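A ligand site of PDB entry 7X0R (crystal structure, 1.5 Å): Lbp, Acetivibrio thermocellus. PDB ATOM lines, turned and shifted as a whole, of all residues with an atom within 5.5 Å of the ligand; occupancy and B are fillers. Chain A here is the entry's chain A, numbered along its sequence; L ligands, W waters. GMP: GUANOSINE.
The side-chain amino group (NZ) of Lys 252 sits at hydrogen-bond distance from an oxygen (O3') of the ligand (2.9 Å). The side-chain sulfur (SD) of Met 160 sits at hydrogen-bond distance from an oxygen (O2') of the ligand, 3.7 Å away. The backbone NH of Gly 34 is in hydrogen-bond range of an oxygen (O6) of the ligand (2.9 Å). N of Gly 214 lies within hydrogen-bond range of O5' of the ligand. The side-chain amide nitrogen (ND2) of Asn 42 sits at hydrogen-bond distance from an oxygen (O6) of the ligand (3.1 Å). An oxygen (O3') of the ligand lies within hydrogen-bond range of the side-chain carboxylate (OD1) of Asp 235 (2.6 Å). The side-chain carboxylate (OD2) of Asp 32 lies within hydrogen-bond range of a nitrogen (N1) of the ligand (2.6 Å). The side-chain carboxylate (OD2) of Asp 113 sits at hydrogen-bond distance from an oxygen (O2') of the ligand (2.8 Å).
N of Ala 213 lies within hydrogen-bond range of ND1 of His 211 (3.0 Å). OD2 of Asp 235 lies within hydrogen-bond range of N of Phe 41 (3.2 Å). The backbone carbonyl oxygen (O) of Phe 188 sits at hydrogen-bond distance from the backbone NH (N) of Gly 215. OD1 of Asn 42 sits at hydrogen-bond distance from N of Asp 32, at 3.4 Å. The backbone carbonyl oxygen (O) of Asp 235 lies within hydrogen-bond range of the backbone NH (N) of Lys 252 (2.9 Å). N of Asn 42 sits at hydrogen-bond distance from OD2 of Asp 38, at 2.8 Å. The side-chain carboxylate (OD1) of Asp 113 lies within salt-bridge range of the side-chain amino group (NZ) of Lys 252 (2.9 Å). The backbone NH (N) of Phe 41 sits at hydrogen-bond distance from the side-chain carboxylate (OD2) of Asp 38.
A nitrogen (N2) of the ligand sits close to the backbone NH of Tyr 91, 3.4 Å away. N of Val 33 touches O6 of the ligand, 3.9 Å away. Phe 41 touches the ligand (CD2 to C5, 3.4 Å). Gly 90 touches the ligand (CA to N2, 3.5 Å). CE of Met 92 touches N2 of the ligand (3.6 Å). CZ of Phe 163 touches O3' of the ligand (3.5 Å). CE1 of Phe 188 touches N9 of the ligand, at 3.4 Å. Ala 212 touches the ligand (C to C5', 3.6 Å). N of Ala 213 touches C5' of the ligand (3.8 Å). Val 234 touches the ligand. Hydrophobic or aromatic side chains within 4 Å of the ligand: Phe 41, Tyr 91, Met 92, Met 160, Phe 163, Phe 188 and Val 234. 18 residues have an atom within 4 Å of the ligand: Asp 32, Val 33, Gly 34, Phe 41, Asn 42, Gly 90, Tyr 91, Met 92, Asp 113, Met 160, Phe 163, Phe 188, Ala 212, Ala 213, Gly 214, Val 234, Asp 235 and Lys 252. The nearest printed residue that does not touch the ligand is Ser 40 (4.4 Å).
Water W2 lies within hydrogen-bond range of OD2 of Asp 113 (2.7 Å), N3 of the ligand (3.0 Å) and N of Tyr 91 (3.0 Å).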
ATOM      1  N   ASP A  32      22.279  24.189  11.741  1.00  0.00           N
ATOM      2  CA  ASP A  32      21.162  25.022  12.105  1.00  0.00           C
ATOM      3  C   ASP A  32      20.208  24.231  12.995  1.00  0.00           C
ATOM      4  O   ASP A  32      20.474  23.105  13.432  1.00  0.00           O
ATOM      5  CB  ASP A  32      20.492  25.531  10.850  1.00  0.00           C
ATOM      6  CG  ASP A  32      20.269  27.001  10.897  1.00  0.00           C
ATOM      7  OD1 ASP A  32      20.973  27.699  11.662  1.00  0.00           O
ATOM      8  OD2 ASP A  32      19.402  27.454  10.162  1.00  0.00           O
ATOM      9  N   VAL A  33      19.060  24.846  13.228  1.00  0.00           N
ATOM     10  CA  VAL A  33      18.079  24.271  14.131  1.00  0.00           C
ATOM     11  C   VAL A  33      17.638  22.889  13.663  1.00  0.00           C
ATOM     12  O   VAL A  33      17.244  22.045  14.484  1.00  0.00           O
ATOM     13  CB  VAL A  33      16.928  25.281  14.300  1.00  0.00           C
ATOM     14  CG1 VAL A  33      17.451  26.494  15.064  1.00  0.00           C
ATOM     15  CG2 VAL A  33      16.413  25.733  12.936  1.00  0.00           C
ATOM     16  N   GLY A  34      17.766  22.601  12.366  1.00  0.00           N
ATOM     17  CA  GLY A  34      17.309  21.321  11.829  1.00  0.00           C
ATOM     18  C   GLY A  34      17.916  20.098  12.505  1.00  0.00           C
ATOM     19  O   GLY A  34      17.231  19.096  12.728  1.00  0.00           O
ATOM     20  N   GLY A  35      19.216  20.135  12.787  1.00  0.00           N
ATOM     21  CA  GLY A  35      19.962  19.013  13.397  1.00  0.00           C
ATOM     22  C   GLY A  35      20.584  18.073  12.384  1.00  0.00           C
ATOM     23  O   GLY A  35      20.088  17.881  11.283  1.00  0.00           O
ATOM     24  N   ASP A  38      18.437  15.204  10.614  1.00  0.00           N
ATOM     25  CA  ASP A  38      17.249  15.681   9.928  1.00  0.00           C
ATOM     26  C   ASP A  38      16.874  14.871   8.692  1.00  0.00           C
ATOM     27  O   ASP A  38      15.840  15.142   8.099  1.00  0.00           O
ATOM     28  CB  ASP A  38      17.345  17.183   9.586  1.00  0.00           C
ATOM     29  CG  ASP A  38      18.426  17.495   8.572  1.00  0.00           C
ATOM     30  OD1 ASP A  38      19.091  16.569   8.080  1.00  0.00           O
ATOM     31  OD2 ASP A  38      18.618  18.697   8.289  1.00  0.00           O
ATOM     32  N   SER A  40      18.069  14.989   5.857  1.00  0.00           N
ATOM     33  CA  SER A  40      18.067  15.844   4.679  1.00  0.00           C
ATOM     34  C   SER A  40      19.277  16.793   4.700  1.00  0.00           C
ATOM     35  O   SER A  40      20.403  16.366   4.538  1.00  0.00           O
ATOM     36  CB  SER A  40      16.733  16.587   4.582  1.00  0.00           C
ATOM     37  OG  SER A  40      16.425  17.275   5.789  1.00  0.00           O
ATOM     38  N   PHE A  41      19.021  18.065   4.969  1.00  0.00           N
ATOM     39  CA  PHE A  41      20.007  19.137   4.725  1.00  0.00           C
ATOM     40  C   PHE A  41      21.232  19.015   5.611  1.00  0.00           C
ATOM     41  O   PHE A  41      22.369  18.873   5.120  1.00  0.00           O
ATOM     42  CB  PHE A  41      19.272  20.457   4.992  1.00  0.00           C
ATOM     43  CG  PHE A  41      20.071  21.695   4.728  1.00  0.00           C
ATOM     44  CD1 PHE A  41      20.547  21.982   3.466  1.00  0.00           C
ATOM     45  CD2 PHE A  41      20.256  22.629   5.744  1.00  0.00           C
ATOM     46  CE1 PHE A  41      21.231  23.174   3.219  1.00  0.00           C
ATOM     47  CE2 PHE A  41      20.923  23.826   5.496  1.00  0.00           C
ATOM     48  CZ  PHE A  41      21.404  24.092   4.246  1.00  0.00           C
ATOM     49  N   ASN A  42      21.051  19.129   6.919  1.00  0.00           N
ATOM     50  CA  ASN A  42      22.199  19.122   7.813  1.00  0.00           C
ATOM     51  C   ASN A  42      22.840  17.757   7.833  1.00  0.00           C
ATOM     52  O   ASN A  42      24.074  17.625   7.929  1.00  0.00           O
ATOM     53  CB  ASN A  42      21.789  19.532   9.231  1.00  0.00           C
ATOM     54  CG  ASN A  42      21.300  20.953   9.301  1.00  0.00           C
ATOM     55  OD1 ASN A  42      22.079  21.908   9.250  1.00  0.00           O
ATOM     56  ND2 ASN A  42      20.008  21.114   9.445  1.00  0.00           N
ATOM     57  N   VAL A  89      26.024  26.091   8.082  1.00  0.00           N
ATOM     58  CA  VAL A  89      25.066  25.388   7.243  1.00  0.00           C
ATOM     59  C   VAL A  89      23.709  26.071   7.399  1.00  0.00           C
ATOM     60  O   VAL A  89      23.005  25.861   8.379  1.00  0.00           O
ATOM     61  CB  VAL A  89      24.997  23.907   7.616  1.00  0.00           C
ATOM     62  CG1 VAL A  89      24.093  23.200   6.698  1.00  0.00           C
ATOM     63  CG2 VAL A  89      26.398  23.317   7.539  1.00  0.00           C
ATOM     64  N   GLY A  90      23.371  26.890   6.423  1.00  0.00           N
ATOM     65  CA  GLY A  90      22.023  27.427   6.338  1.00  0.00           C
ATOM     66  C   GLY A  90      22.005  28.935   6.256  1.00  0.00           C
ATOM     67  O   GLY A  90      22.864  29.620   6.822  1.00  0.00           O
ATOM     68  N   TYR A  91      20.985  29.467   5.602  1.00  0.00           N
ATOM     69  CA  TYR A  91      20.968  30.900   5.326  1.00  0.00           C
ATOM     70  C   TYR A  91      20.793  31.742   6.592  1.00  0.00           C
ATOM     71  O   TYR A  91      21.189  32.902   6.619  1.00  0.00           O
ATOM     72  CB  TYR A  91      19.889  31.260   4.298  1.00  0.00           C
ATOM     73  CG  TYR A  91      18.476  31.083   4.782  1.00  0.00           C
ATOM     74  CD1 TYR A  91      17.801  32.109   5.446  1.00  0.00           C
ATOM     75  CD2 TYR A  91      17.790  29.890   4.578  1.00  0.00           C
ATOM     76  CE1 TYR A  91      16.518  31.940   5.901  1.00  0.00           C
ATOM     77  CE2 TYR A  91      16.503  29.728   5.038  1.00  0.00           C
ATOM     78  CZ  TYR A  91      15.873  30.745   5.698  1.00  0.00           C
ATOM     79  OH  TYR A  91      14.562  30.581   6.159  1.00  0.00           O
ATOM     80  N   MET A  92      20.175  31.182   7.649  1.00  0.00           N
ATOM     81  CA  MET A  92      19.928  31.943   8.868  1.00  0.00           C
ATOM     82  C   MET A  92      21.190  32.263   9.628  1.00  0.00           C
ATOM     83  O   MET A  92      21.158  33.129  10.497  1.00  0.00           O
ATOM     84  CB  MET A  92      18.926  31.195   9.754  1.00  0.00           C
ATOM     85  CG  MET A  92      17.534  31.270   9.168  1.00  0.00           C
ATOM     86  SD  MET A  92      16.244  30.611  10.212  1.00  0.00           S
ATOM     87  CE  MET A  92      16.699  28.874  10.201  1.00  0.00           C
ATOM     88  N   ASP A 113      23.874  28.447   1.298  1.00  0.00           N
ATOM     89  CA  ASP A 113      22.557  28.986   0.966  1.00  0.00           C
ATOM     90  C   ASP A 113      22.427  30.493   1.187  1.00  0.00           C
ATOM     91  O   ASP A 113      21.288  31.026   1.171  1.00  0.00           O
ATOM     92  CB  ASP A 113      21.385  28.321   1.699  1.00  0.00           C
ATOM     93  CG  ASP A 113      21.009  26.936   1.145  1.00  0.00           C
ATOM     94  OD1 ASP A 113      21.415  26.551   0.034  1.00  0.00           O
ATOM     95  OD2 ASP A 113      20.241  26.227   1.850  1.00  0.00           O
ATOM     96  N   GLN A 129      18.420  25.440  -6.510  1.00  0.00           N
ATOM     97  CA  GLN A 129      17.367  24.514  -6.054  1.00  0.00           C
ATOM     98  C   GLN A 129      16.093  24.700  -6.861  1.00  0.00           C
ATOM     99  O   GLN A 129      15.342  23.801  -6.910  1.00  0.00           O
ATOM    100  CB  GLN A 129      17.131  24.678  -4.548  1.00  0.00           C
ATOM    101  CG  GLN A 129      16.735  26.075  -4.135  1.00  0.00           C
ATOM    102  CD  GLN A 129      17.840  26.712  -3.344  1.00  0.00           C
ATOM    103  OE1 GLN A 129      18.547  26.037  -2.623  1.00  0.00           O
ATOM    104  NE2 GLN A 129      17.996  28.016  -3.514  1.00  0.00           N
ATOM    105  N   MET A 160      14.343  30.015   0.236  1.00  0.00           N
ATOM    106  CA  MET A 160      13.306  29.017   0.382  1.00  0.00           C
ATOM    107  C   MET A 160      12.233  29.167  -0.684  1.00  0.00           C
ATOM    108  O   MET A 160      11.699  28.173  -1.173  1.00  0.00           O
ATOM    109  CB  MET A 160      12.700  29.069   1.780  1.00  0.00           C
ATOM    110  CG  MET A 160      13.715  28.765   2.917  1.00  0.00           C
ATOM    111  SD  MET A 160      14.652  27.239   2.571  1.00  0.00           S
ATOM    112  CE  MET A 160      13.297  26.072   2.434  1.00  0.00           C
ATOM    113  N   PHE A 163      12.499  27.181  -3.952  1.00  0.00           N
ATOM    114  CA  PHE A 163      11.905  25.854  -4.021  1.00  0.00           C
ATOM    115  C   PHE A 163      10.451  25.956  -4.476  1.00  0.00           C
ATOM    116  O   PHE A 163       9.981  25.190  -5.324  1.00  0.00           O
ATOM    117  CB  PHE A 163      11.941  25.179  -2.646  1.00  0.00           C
ATOM    118  CG  PHE A 163      13.280  24.684  -2.208  1.00  0.00           C
ATOM    119  CD1 PHE A 163      13.735  23.430  -2.588  1.00  0.00           C
ATOM    120  CD2 PHE A 163      14.050  25.430  -1.359  1.00  0.00           C
ATOM    121  CE1 PHE A 163      14.953  22.970  -2.167  1.00  0.00           C
ATOM    122  CE2 PHE A 163      15.273  24.956  -0.899  1.00  0.00           C
ATOM    123  CZ  PHE A 163      15.726  23.733  -1.300  1.00  0.00           C
ATOM    124  N   PHE A 188      12.254  24.129  10.690  1.00  0.00           N
ATOM    125  CA  PHE A 188      12.945  23.049  10.017  1.00  0.00           C
ATOM    126  C   PHE A 188      13.106  21.834  10.911  1.00  0.00           C
ATOM    127  O   PHE A 188      13.762  20.857  10.511  1.00  0.00           O
ATOM    128  CB  PHE A 188      14.336  23.534   9.561  1.00  0.00           C
ATOM    129  CG  PHE A 188      14.281  24.513   8.419  1.00  0.00           C
ATOM    130  CD1 PHE A 188      13.842  24.135   7.167  1.00  0.00           C
ATOM    131  CD2 PHE A 188      14.700  25.824   8.600  1.00  0.00           C
ATOM    132  CE1 PHE A 188      13.816  25.048   6.114  1.00  0.00           C
ATOM    133  CE2 PHE A 188      14.667  26.731   7.548  1.00  0.00           C
ATOM    134  CZ  PHE A 188      14.234  26.333   6.307  1.00  0.00           C
ATOM    135  N   HIS A 211       8.126  18.371   0.180  1.00  0.00           N
ATOM    136  CA  HIS A 211       8.578  19.244   1.256  1.00  0.00           C
ATOM    137  C   HIS A 211       9.938  19.831   0.936  1.00  0.00           C
ATOM    138  O   HIS A 211      10.804  19.166   0.355  1.00  0.00           O
ATOM    139  CB  HIS A 211       8.608  18.526   2.627  1.00  0.00           C
ATOM    140  CG  HIS A 211       9.874  17.780   2.906  1.00  0.00           C
ATOM    141  ND1 HIS A 211      10.964  18.376   3.503  1.00  0.00           N
ATOM    142  CD2 HIS A 211      10.221  16.499   2.669  1.00  0.00           C
ATOM    143  CE1 HIS A 211      11.944  17.493   3.593  1.00  0.00           C
ATOM    144  NE2 HIS A 211      11.512  16.338   3.100  1.00  0.00           N
ATOM    145  N   ALA A 212      10.122  21.080   1.324  1.00  0.00           N
ATOM    146  CA  ALA A 212      11.449  21.703   1.416  1.00  0.00           C
ATOM    147  C   ALA A 212      11.541  22.244   2.830  1.00  0.00           C
ATOM    148  O   ALA A 212      11.469  23.453   3.058  1.00  0.00           O
ATOM    149  CB  ALA A 212      11.628  22.783   0.377  1.00  0.00           C
ATOM    150  N   ALA A 213      11.632  21.324   3.784  1.00  0.00           N
ATOM    151  CA  ALA A 213      11.411  21.671   5.182  1.00  0.00           C
ATOM    152  C   ALA A 213      12.359  20.955   6.133  1.00  0.00           C
ATOM    153  O   ALA A 213      12.089  20.885   7.346  1.00  0.00           O
ATOM    154  CB  ALA A 213       9.968  21.382   5.583  1.00  0.00           C
ATOM    155  N   GLY A 214      13.477  20.443   5.620  1.00  0.00           N
ATOM    156  CA  GLY A 214      14.442  19.840   6.516  1.00  0.00           C
ATOM    157  C   GLY A 214      13.832  18.753   7.356  1.00  0.00           C
ATOM    158  O   GLY A 214      13.067  17.901   6.860  1.00  0.00           O
ATOM    159  N   GLY A 215      14.154  18.768   8.643  1.00  0.00           N
ATOM    160  CA  GLY A 215      13.684  17.728   9.539  1.00  0.00           C
ATOM    161  C   GLY A 215      12.179  17.669   9.674  1.00  0.00           C
ATOM    162  O   GLY A 215      11.613  16.609   9.942  1.00  0.00           O
ATOM    163  N   VAL A 234      13.741  15.791  -0.394  1.00  0.00           N
ATOM    164  CA  VAL A 234      14.600  16.932  -0.684  1.00  0.00           C
ATOM    165  C   VAL A 234      15.983  16.694  -0.082  1.00  0.00           C
ATOM    166  O   VAL A 234      16.131  15.950   0.896  1.00  0.00           O
ATOM    167  CB  VAL A 234      13.961  18.250  -0.177  1.00  0.00           C
ATOM    168  CG1 VAL A 234      14.102  18.346   1.329  1.00  0.00           C
ATOM    169  CG2 VAL A 234      14.544  19.496  -0.895  1.00  0.00           C
ATOM    170  N   ASP A 235      16.993  17.349  -0.684  1.00  0.00           N
ATOM    171  CA  ASP A 235      18.388  17.392  -0.279  1.00  0.00           C
ATOM    172  C   ASP A 235      19.105  16.094  -0.624  1.00  0.00           C
ATOM    173  O   ASP A 235      19.998  16.064  -1.471  1.00  0.00           O
ATOM    174  CB  ASP A 235      18.544  17.740   1.210  1.00  0.00           C
ATOM    175  CG  ASP A 235      18.046  19.128   1.514  1.00  0.00           C
ATOM    176  OD1 ASP A 235      18.288  20.035   0.705  1.00  0.00           O
ATOM    177  OD2 ASP A 235      17.365  19.284   2.524  1.00  0.00           O
ATOM    178  N   LYS A 252      20.048  18.149  -3.442  1.00  0.00           N
ATOM    179  CA  LYS A 252      20.916  19.314  -3.288  1.00  0.00           C
ATOM    180  C   LYS A 252      22.151  18.798  -2.584  1.00  0.00           C
ATOM    181  O   LYS A 252      22.095  18.421  -1.405  1.00  0.00           O
ATOM    182  CB  LYS A 252      20.187  20.360  -2.476  1.00  0.00           C
ATOM    183  CG  LYS A 252      20.936  21.591  -2.179  1.00  0.00           C
ATOM    184  CD  LYS A 252      19.884  22.607  -1.720  1.00  0.00           C
ATOM    185  CE  LYS A 252      20.434  23.476  -0.685  1.00  0.00           C
ATOM    186  NZ  LYS A 252      19.415  24.484  -0.369  1.00  0.00           N
HETATM  187  O5' GMP L   1      15.374  20.756   3.387  1.00  0.00           O
HETATM  188  C5' GMP L   1      15.068  21.584   2.263  1.00  0.00           C
HETATM  189  C4' GMP L   1      15.852  22.879   2.313  1.00  0.00           C
HETATM  190  O4' GMP L   1      15.457  23.636   3.488  1.00  0.00           O
HETATM  191  C3' GMP L   1      17.354  22.772   2.435  1.00  0.00           C
HETATM  192  O3' GMP L   1      17.968  22.559   1.156  1.00  0.00           O
HETATM  193  C2' GMP L   1      17.684  24.157   2.953  1.00  0.00           C
HETATM  194  O2' GMP L   1      17.636  25.162   1.965  1.00  0.00           O
HETATM  195  C1' GMP L   1      16.559  24.352   3.962  1.00  0.00           C
HETATM  196  N9  GMP L   1      16.891  23.935   5.330  1.00  0.00           N
HETATM  197  C8  GMP L   1      16.611  22.662   5.666  1.00  0.00           C
HETATM  198  N7  GMP L   1      16.984  22.520   6.976  1.00  0.00           N
HETATM  199  C5  GMP L   1      17.459  23.699   7.384  1.00  0.00           C
HETATM  200  C6  GMP L   1      18.045  24.251   8.648  1.00  0.00           C
HETATM  201  O6  GMP L   1      18.164  23.576   9.624  1.00  0.00           O
HETATM  202  N1  GMP L   1      18.431  25.622   8.617  1.00  0.00           N
HETATM  203  C2  GMP L   1      18.312  26.448   7.452  1.00  0.00           C
HETATM  204  N2  GMP L   1      18.689  27.834   7.433  1.00  0.00           N
HETATM  205  N3  GMP L   1      17.775  25.913   6.243  1.00  0.00           N
HETATM  206  C4  GMP L   1      17.387  24.525   6.329  1.00  0.00           C
HETATM  207  O   HOH W   1      16.670  20.471   8.935  1.00  0.00           O
HETATM  208  O   HOH W   2      19.501  27.211   4.203  1.00  0.00           O
